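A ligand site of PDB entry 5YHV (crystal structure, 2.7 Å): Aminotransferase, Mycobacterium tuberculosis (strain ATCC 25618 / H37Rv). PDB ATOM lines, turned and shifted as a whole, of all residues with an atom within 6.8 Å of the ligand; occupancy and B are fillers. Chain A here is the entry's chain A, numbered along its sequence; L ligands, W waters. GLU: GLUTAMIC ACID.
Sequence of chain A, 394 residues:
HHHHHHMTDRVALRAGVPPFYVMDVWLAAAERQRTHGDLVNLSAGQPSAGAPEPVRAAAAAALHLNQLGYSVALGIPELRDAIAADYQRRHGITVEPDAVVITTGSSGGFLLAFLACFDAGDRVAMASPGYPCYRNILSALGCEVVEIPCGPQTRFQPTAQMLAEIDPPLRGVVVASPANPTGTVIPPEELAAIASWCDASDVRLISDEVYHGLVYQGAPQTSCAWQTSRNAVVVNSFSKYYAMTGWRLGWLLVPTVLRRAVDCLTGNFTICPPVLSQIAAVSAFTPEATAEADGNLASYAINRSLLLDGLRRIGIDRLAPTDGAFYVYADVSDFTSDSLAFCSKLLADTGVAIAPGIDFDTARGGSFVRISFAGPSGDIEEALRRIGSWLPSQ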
ATOM      1  N   ASP A  86     -22.252  -9.709 -25.557  1.00  0.00           N
ATOM      2  CA  ASP A  86     -22.312  -8.676 -24.514  1.00  0.00           C
ATOM      3  C   ASP A  86     -23.729  -8.518 -23.950  1.00  0.00           C
ATOM      4  O   ASP A  86     -23.882  -8.261 -22.747  1.00  0.00           O
ATOM      5  CB  ASP A  86     -21.790  -7.334 -25.053  1.00  0.00           C
ATOM      6  CG  ASP A  86     -21.672  -6.275 -23.959  1.00  0.00           C
ATOM      7  OD1 ASP A  86     -20.860  -6.457 -23.037  1.00  0.00           O
ATOM      8  OD2 ASP A  86     -22.379  -5.246 -24.052  1.00  0.00           O
ATOM      9  N   TYR A  87     -24.734  -8.670 -24.805  1.00  0.00           N
ATOM     10  CA  TYR A  87     -26.148  -8.650 -24.392  1.00  0.00           C
ATOM     11  C   TYR A  87     -26.488  -9.790 -23.435  1.00  0.00           C
ATOM     12  O   TYR A  87     -27.283  -9.602 -22.507  1.00  0.00           O
ATOM     13  CB  TYR A  87     -27.073  -8.699 -25.614  1.00  0.00           C
ATOM     14  CG  TYR A  87     -27.270  -7.353 -26.284  1.00  0.00           C
ATOM     15  CD1 TYR A  87     -28.200  -6.421 -25.794  1.00  0.00           C
ATOM     16  CD2 TYR A  87     -26.527  -7.013 -27.425  1.00  0.00           C
ATOM     17  CE1 TYR A  87     -28.373  -5.193 -26.406  1.00  0.00           C
ATOM     18  CE2 TYR A  87     -26.701  -5.784 -28.051  1.00  0.00           C
ATOM     19  CZ  TYR A  87     -27.612  -4.879 -27.535  1.00  0.00           C
ATOM     20  OH  TYR A  87     -27.772  -3.660 -28.163  1.00  0.00           O
ATOM     21  N   HIS A  91     -26.470  -8.426 -19.633  1.00  0.00           N
ATOM     22  CA  HIS A  91     -27.905  -8.115 -19.486  1.00  0.00           C
ATOM     23  C   HIS A  91     -28.868  -9.305 -19.650  1.00  0.00           C
ATOM     24  O   HIS A  91     -30.093  -9.128 -19.592  1.00  0.00           O
ATOM     25  CB  HIS A  91     -28.288  -6.967 -20.424  1.00  0.00           C
ATOM     26  CG  HIS A  91     -27.239  -5.906 -20.524  1.00  0.00           C
ATOM     27  ND1 HIS A  91     -27.029  -4.972 -19.531  1.00  0.00           N
ATOM     28  CD2 HIS A  91     -26.303  -5.662 -21.479  1.00  0.00           C
ATOM     29  CE1 HIS A  91     -26.015  -4.192 -19.874  1.00  0.00           C
ATOM     30  NE2 HIS A  91     -25.559  -4.591 -21.047  1.00  0.00           N
ATOM     31  N   GLU A 209     -30.614   3.567 -27.544  1.00  0.00           N
ATOM     32  CA  GLU A 209     -30.022   2.990 -26.349  1.00  0.00           C
ATOM     33  C   GLU A 209     -28.523   3.350 -26.275  1.00  0.00           C
ATOM     34  O   GLU A 209     -27.727   2.654 -25.657  1.00  0.00           O
ATOM     35  CB  GLU A 209     -30.277   1.488 -26.314  1.00  0.00           C
ATOM     36  CG  GLU A 209     -31.763   1.112 -26.284  1.00  0.00           C
ATOM     37  CD  GLU A 209     -32.023  -0.378 -26.170  1.00  0.00           C
ATOM     38  OE1 GLU A 209     -31.082  -1.153 -25.918  1.00  0.00           O
ATOM     39  OE2 GLU A 209     -33.193  -0.783 -26.346  1.00  0.00           O
ATOM     40  N   VAL A 210     -28.186   4.481 -26.891  1.00  0.00           N
ATOM     41  CA  VAL A 210     -26.824   4.998 -27.061  1.00  0.00           C
ATOM     42  C   VAL A 210     -26.099   5.248 -25.722  1.00  0.00           C
ATOM     43  O   VAL A 210     -24.898   4.970 -25.605  1.00  0.00           O
ATOM     44  CB  VAL A 210     -26.838   6.270 -27.962  1.00  0.00           C
ATOM     45  CG1 VAL A 210     -25.493   7.003 -27.981  1.00  0.00           C
ATOM     46  CG2 VAL A 210     -27.240   5.889 -29.377  1.00  0.00           C
ATOM     47  N   TYR A 211     -26.828   5.731 -24.720  1.00  0.00           N
ATOM     48  CA  TYR A 211     -26.230   6.059 -23.421  1.00  0.00           C
ATOM     49  C   TYR A 211     -26.272   4.932 -22.375  1.00  0.00           C
ATOM     50  O   TYR A 211     -25.897   5.141 -21.220  1.00  0.00           O
ATOM     51  CB  TYR A 211     -26.838   7.342 -22.861  1.00  0.00           C
ATOM     52  CG  TYR A 211     -26.376   8.583 -23.581  1.00  0.00           C
ATOM     53  CD1 TYR A 211     -25.154   9.186 -23.249  1.00  0.00           C
ATOM     54  CD2 TYR A 211     -27.143   9.139 -24.598  1.00  0.00           C
ATOM     55  CE1 TYR A 211     -24.728  10.335 -23.907  1.00  0.00           C
ATOM     56  CE2 TYR A 211     -26.715  10.281 -25.264  1.00  0.00           C
ATOM     57  CZ  TYR A 211     -25.512  10.878 -24.919  1.00  0.00           C
ATOM     58  OH  TYR A 211     -25.098  11.999 -25.572  1.00  0.00           O
ATOM     59  N   HIS A 212     -26.709   3.745 -22.795  1.00  0.00           N
ATOM     60  CA  HIS A 212     -26.651   2.539 -21.958  1.00  0.00           C
ATOM     61  C   HIS A 212     -25.229   2.300 -21.456  1.00  0.00           C
ATOM     62  O   HIS A 212     -24.260   2.493 -22.197  1.00  0.00           O
ATOM     63  CB  HIS A 212     -27.127   1.330 -22.757  1.00  0.00           C
ATOM     64  CG  HIS A 212     -28.614   1.171 -22.802  1.00  0.00           C
ATOM     65  ND1 HIS A 212     -29.234  -0.057 -22.825  1.00  0.00           N
ATOM     66  CD2 HIS A 212     -29.606   2.099 -22.837  1.00  0.00           C
ATOM     67  CE1 HIS A 212     -30.541   0.121 -22.866  1.00  0.00           C
ATOM     68  NE2 HIS A 212     -30.797   1.412 -22.880  1.00  0.00           N
ATOM     69  N   GLY A 213     -25.123   1.909 -20.191  1.00  0.00           N
ATOM     70  CA  GLY A 213     -23.824   1.755 -19.530  1.00  0.00           C
ATOM     71  C   GLY A 213     -23.444   2.969 -18.708  1.00  0.00           C
ATOM     72  O   GLY A 213     -22.596   2.876 -17.819  1.00  0.00           O
ATOM     73  N   LEU A 214     -24.047   4.113 -19.017  1.00  0.00           N
ATOM     74  CA  LEU A 214     -23.819   5.349 -18.276  1.00  0.00           C
ATOM     75  C   LEU A 214     -25.065   5.689 -17.474  1.00  0.00           C
ATOM     76  O   LEU A 214     -25.902   6.506 -17.886  1.00  0.00           O
ATOM     77  CB  LEU A 214     -23.426   6.489 -19.218  1.00  0.00           C
ATOM     78  CG  LEU A 214     -22.132   6.443 -20.053  1.00  0.00           C
ATOM     79  CD1 LEU A 214     -21.978   7.674 -20.933  1.00  0.00           C
ATOM     80  CD2 LEU A 214     -20.878   6.218 -19.206  1.00  0.00           C
ATOM     81  N   THR A 222     -31.904   0.409 -16.542  1.00  0.00           N
ATOM     82  CA  THR A 222     -31.956   0.562 -17.983  1.00  0.00           C
ATOM     83  C   THR A 222     -32.319  -0.823 -18.553  1.00  0.00           C
ATOM     84  O   THR A 222     -31.996  -1.857 -17.936  1.00  0.00           O
ATOM     85  CB  THR A 222     -30.565   1.105 -18.435  1.00  0.00           C
ATOM     86  OG1 THR A 222     -30.631   2.073 -19.489  1.00  0.00           O
ATOM     87  CG2 THR A 222     -29.590   0.006 -18.646  1.00  0.00           C
ATOM     88  N   SER A 223     -33.026  -0.838 -19.682  1.00  0.00           N
ATOM     89  CA  SER A 223     -33.491  -2.058 -20.290  1.00  0.00           C
ATOM     90  C   SER A 223     -33.508  -1.945 -21.807  1.00  0.00           C
ATOM     91  O   SER A 223     -33.665  -0.846 -22.355  1.00  0.00           O
ATOM     92  CB  SER A 223     -34.882  -2.430 -19.763  1.00  0.00           C
ATOM     93  OG  SER A 223     -35.793  -1.351 -19.868  1.00  0.00           O
ATOM     94  N   CYS A 224     -33.298  -3.079 -22.466  1.00  0.00           N
ATOM     95  CA  CYS A 224     -33.336  -3.144 -23.916  1.00  0.00           C
ATOM     96  C   CYS A 224     -34.780  -3.386 -24.362  1.00  0.00           C
ATOM     97  O   CYS A 224     -35.510  -4.155 -23.737  1.00  0.00           O
ATOM     98  CB  CYS A 224     -32.426  -4.251 -24.432  1.00  0.00           C
ATOM     99  SG  CYS A 224     -32.394  -4.353 -26.222  1.00  0.00           S
ATOM    100  N   GLN A 227     -36.132  -6.933 -24.731  1.00  0.00           N
ATOM    101  CA  GLN A 227     -36.626  -7.682 -23.574  1.00  0.00           C
ATOM    102  C   GLN A 227     -38.134  -7.908 -23.676  1.00  0.00           C
ATOM    103  O   GLN A 227     -38.627  -8.931 -23.196  1.00  0.00           O
ATOM    104  CB  GLN A 227     -36.255  -6.986 -22.267  1.00  0.00           C
ATOM    105  CG  GLN A 227     -34.773  -7.069 -21.934  1.00  0.00           C
ATOM    106  CD  GLN A 227     -34.385  -6.357 -20.662  1.00  0.00           C
ATOM    107  OE1 GLN A 227     -33.478  -5.523 -20.649  1.00  0.00           O
ATOM    108  NE2 GLN A 227     -35.063  -6.702 -19.565  1.00  0.00           N
ATOM    109  N   VAL A 234     -33.333  -1.412 -32.336  1.00  0.00           N
ATOM    110  CA  VAL A 234     -32.448  -0.911 -31.278  1.00  0.00           C
ATOM    111  C   VAL A 234     -31.274  -0.196 -31.929  1.00  0.00           C
ATOM    112  O   VAL A 234     -30.625  -0.731 -32.821  1.00  0.00           O
ATOM    113  CB  VAL A 234     -31.949  -2.058 -30.363  1.00  0.00           C
ATOM    114  CG1 VAL A 234     -30.938  -1.561 -29.321  1.00  0.00           C
ATOM    115  CG2 VAL A 234     -33.116  -2.765 -29.689  1.00  0.00           C
ATOM    116  N   ASN A 236     -27.658   1.714 -31.022  1.00  0.00           N
ATOM    117  CA  ASN A 236     -26.611   1.891 -30.008  1.00  0.00           C
ATOM    118  C   ASN A 236     -25.294   2.307 -30.666  1.00  0.00           C
ATOM    119  O   ASN A 236     -25.156   2.271 -31.888  1.00  0.00           O
ATOM    120  CB  ASN A 236     -26.444   0.602 -29.196  1.00  0.00           C
ATOM    121  CG  ASN A 236     -26.070   0.865 -27.737  1.00  0.00           C
ATOM    122  OD1 ASN A 236     -25.297   1.780 -27.422  1.00  0.00           O
ATOM    123  ND2 ASN A 236     -26.623   0.053 -26.842  1.00  0.00           N
ATOM    124  N   SER A 237     -24.322   2.705 -29.840  1.00  0.00           N
ATOM    125  CA  SER A 237     -23.067   3.285 -30.329  1.00  0.00           C
ATOM    126  C   SER A 237     -21.881   2.973 -29.420  1.00  0.00           C
ATOM    127  O   SER A 237     -22.054   2.612 -28.261  1.00  0.00           O
ATOM    128  CB  SER A 237     -23.222   4.801 -30.477  1.00  0.00           C
ATOM    129  OG  SER A 237     -22.037   5.370 -31.002  1.00  0.00           O
ATOM    130  N   PHE A 238     -20.686   3.134 -29.989  1.00  0.00           N
ATOM    131  CA  PHE A 238     -19.430   3.082 -29.223  1.00  0.00           C
ATOM    132  C   PHE A 238     -19.005   4.478 -28.773  1.00  0.00           C
ATOM    133  O   PHE A 238     -17.995   4.621 -28.090  1.00  0.00           O
ATOM    134  CB  PHE A 238     -18.321   2.438 -30.070  1.00  0.00           C
ATOM    135  CG  PHE A 238     -18.499   0.973 -30.289  1.00  0.00           C
ATOM    136  CD1 PHE A 238     -18.028   0.052 -29.349  1.00  0.00           C
ATOM    137  CD2 PHE A 238     -19.148   0.494 -31.433  1.00  0.00           C
ATOM    138  CE1 PHE A 238     -18.194  -1.316 -29.536  1.00  0.00           C
ATOM    139  CE2 PHE A 238     -19.303  -0.878 -31.628  1.00  0.00           C
ATOM    140  CZ  PHE A 238     -18.828  -1.776 -30.679  1.00  0.00           C
ATOM    141  N   TYR A 241     -20.429   5.412 -24.129  1.00  0.00           N
ATOM    142  CA  TYR A 241     -19.957   4.551 -23.055  1.00  0.00           C
ATOM    143  C   TYR A 241     -18.496   4.158 -23.260  1.00  0.00           C
ATOM    144  O   TYR A 241     -17.704   4.213 -22.320  1.00  0.00           O
ATOM    145  CB  TYR A 241     -20.849   3.315 -22.883  1.00  0.00           C
ATOM    146  CG  TYR A 241     -20.318   2.330 -21.866  1.00  0.00           C
ATOM    147  CD1 TYR A 241     -20.300   2.636 -20.503  1.00  0.00           C
ATOM    148  CD2 TYR A 241     -19.830   1.089 -22.269  1.00  0.00           C
ATOM    149  CE1 TYR A 241     -19.804   1.738 -19.561  1.00  0.00           C
ATOM    150  CE2 TYR A 241     -19.339   0.176 -21.343  1.00  0.00           C
ATOM    151  CZ  TYR A 241     -19.328   0.505 -19.999  1.00  0.00           C
ATOM    152  OH  TYR A 241     -18.840  -0.401 -19.080  1.00  0.00           O
ATOM    153  N   TYR A 242     -18.148   3.808 -24.498  1.00  0.00           N
ATOM    154  CA  TYR A 242     -16.783   3.431 -24.843  1.00  0.00           C
ATOM    155  C   TYR A 242     -15.914   4.590 -25.321  1.00  0.00           C
ATOM    156  O   TYR A 242     -14.767   4.383 -25.723  1.00  0.00           O
ATOM    157  CB  TYR A 242     -16.770   2.275 -25.842  1.00  0.00           C
ATOM    158  CG  TYR A 242     -17.089   0.945 -25.198  1.00  0.00           C
ATOM    159  CD1 TYR A 242     -16.238   0.392 -24.238  1.00  0.00           C
ATOM    160  CD2 TYR A 242     -18.247   0.237 -25.549  1.00  0.00           C
ATOM    161  CE1 TYR A 242     -16.531  -0.814 -23.631  1.00  0.00           C
ATOM    162  CE2 TYR A 242     -18.545  -0.984 -24.958  1.00  0.00           C
ATOM    163  CZ  TYR A 242     -17.684  -1.505 -23.995  1.00  0.00           C
ATOM    164  OH  TYR A 242     -17.965  -2.714 -23.395  1.00  0.00           O
ATOM    165  N   TRP A 251     -23.958   0.188 -33.729  1.00  0.00           N
ATOM    166  CA  TRP A 251     -24.692  -0.978 -34.214  1.00  0.00           C
ATOM    167  C   TRP A 251     -26.204  -0.860 -34.080  1.00  0.00           C
ATOM    168  O   TRP A 251     -26.718  -0.039 -33.323  1.00  0.00           O
ATOM    169  CB  TRP A 251     -24.176  -2.271 -33.542  1.00  0.00           C
ATOM    170  CG  TRP A 251     -24.588  -2.446 -32.111  1.00  0.00           C
ATOM    171  CD1 TRP A 251     -25.701  -3.076 -31.651  1.00  0.00           C
ATOM    172  CD2 TRP A 251     -23.879  -1.994 -30.956  1.00  0.00           C
ATOM    173  NE1 TRP A 251     -25.743  -3.056 -30.276  1.00  0.00           N
ATOM    174  CE2 TRP A 251     -24.625  -2.394 -29.822  1.00  0.00           C
ATOM    175  CE3 TRP A 251     -22.676  -1.284 -30.762  1.00  0.00           C
ATOM    176  CZ2 TRP A 251     -24.222  -2.112 -28.510  1.00  0.00           C
ATOM    177  CZ3 TRP A 251     -22.275  -0.995 -29.457  1.00  0.00           C
ATOM    178  CH2 TRP A 251     -23.037  -1.411 -28.353  1.00  0.00           C
ATOM    179  N   PHE A 285     -14.611  -5.061 -25.560  1.00  0.00           N
ATOM    180  CA  PHE A 285     -15.291  -6.039 -24.723  1.00  0.00           C
ATOM    181  C   PHE A 285     -14.337  -6.857 -23.843  1.00  0.00           C
ATOM    182  O   PHE A 285     -14.710  -7.902 -23.303  1.00  0.00           O
ATOM    183  CB  PHE A 285     -16.211  -6.914 -25.593  1.00  0.00           C
ATOM    184  CG  PHE A 285     -17.253  -6.124 -26.333  1.00  0.00           C
ATOM    185  CD1 PHE A 285     -18.421  -5.690 -25.686  1.00  0.00           C
ATOM    186  CD2 PHE A 285     -17.061  -5.781 -27.678  1.00  0.00           C
ATOM    187  CE1 PHE A 285     -19.367  -4.942 -26.381  1.00  0.00           C
ATOM    188  CE2 PHE A 285     -18.017  -5.037 -28.360  1.00  0.00           C
ATOM    189  CZ  PHE A 285     -19.161  -4.611 -27.714  1.00  0.00           C
HETATM  190  N   GLU L   1     -26.669  -1.589 -21.071  1.00  0.00           N
HETATM  191  CA  GLU L   1     -26.219  -1.641 -22.499  1.00  0.00           C
HETATM  192  C   GLU L   1     -27.066  -2.551 -23.388  1.00  0.00           C
HETATM  193  O   GLU L   1     -28.200  -2.900 -23.032  1.00  0.00           O
HETATM  194  CB  GLU L   1     -24.731  -1.991 -22.615  1.00  0.00           C
HETATM  195  CG  GLU L   1     -23.849  -0.813 -22.963  1.00  0.00           C
HETATM  196  CD  GLU L   1     -22.849  -1.152 -24.046  1.00  0.00           C
HETATM  197  OE1 GLU L   1     -22.068  -2.115 -23.869  1.00  0.00           O
HETATM  198  OE2 GLU L   1     -22.853  -0.457 -25.080  1.00  0.00           O
HETATM  199  OXT GLU L   1     -26.660  -2.929 -24.487  1.00  0.00           O
HETATM  200  O   HOH W   1     -28.697  -1.885 -26.415  1.00  0.00           O
HETATM  201  O   HOH W   2     -29.980  -4.072 -21.141  1.00  0.00           O
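OE1 of the ligand lies close to OD2 of Asp 86, at 3.2 Å. Tyr 87 touches the ligand. N of Gly 213 touches N of the ligand (3.9 Å). ND2 of Asn 236 touches OXT of the ligand (3.8 Å). Tyr 242 touches the ligand (CE2 to OE1, 3.9 Å). CH2 of Trp 251 touches OE2 of the ligand, 3.4 Å away. Hydrophobic or aromatic side chains that line the ligand: Tyr 87, His 91, His 212, Tyr 242 and Trp 251. Along chain A the residues within 4 Å of the ligand span positions 86 to 251. The nearest printed residue that does not touch the ligand is Thr 222 (4.1 Å).
NE2 of His 91 lies close to N of the ligand. A ring nitrogen (ND1) of His 212 lies within hydrogen-bond range of an oxygen (O) of the ligand, 3.0 Å away.
The side-chain hydroxyl of Tyr 87 is in hydrogen-bond range of the indole nitrogen of Trp 251, at 3.0 Å. A ring nitrogen (NE2) of His 212 is in hydrogen-bond range of the side-chain hydroxyl of Thr 222 (3.5 Å). The side-chain amide nitrogen of Asn 236 sits at hydrogen-bond distance from the backbone carbonyl oxygen of Glu 209, at 3.1 Å. The backbone NH of Trp 251 lies within hydrogen-bond range of the backbone carbonyl oxygen of Asn 236, at 3.0 Å.
Water W2 bridges O of the ligand (2.8 Å) and ND1 of His 91 (3.5 Å). Water W1 lies within hydrogen-bond range of OE1 of Glu 209, OH of Tyr 87, ND2 of Asn 236 and OXT of the ligand.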
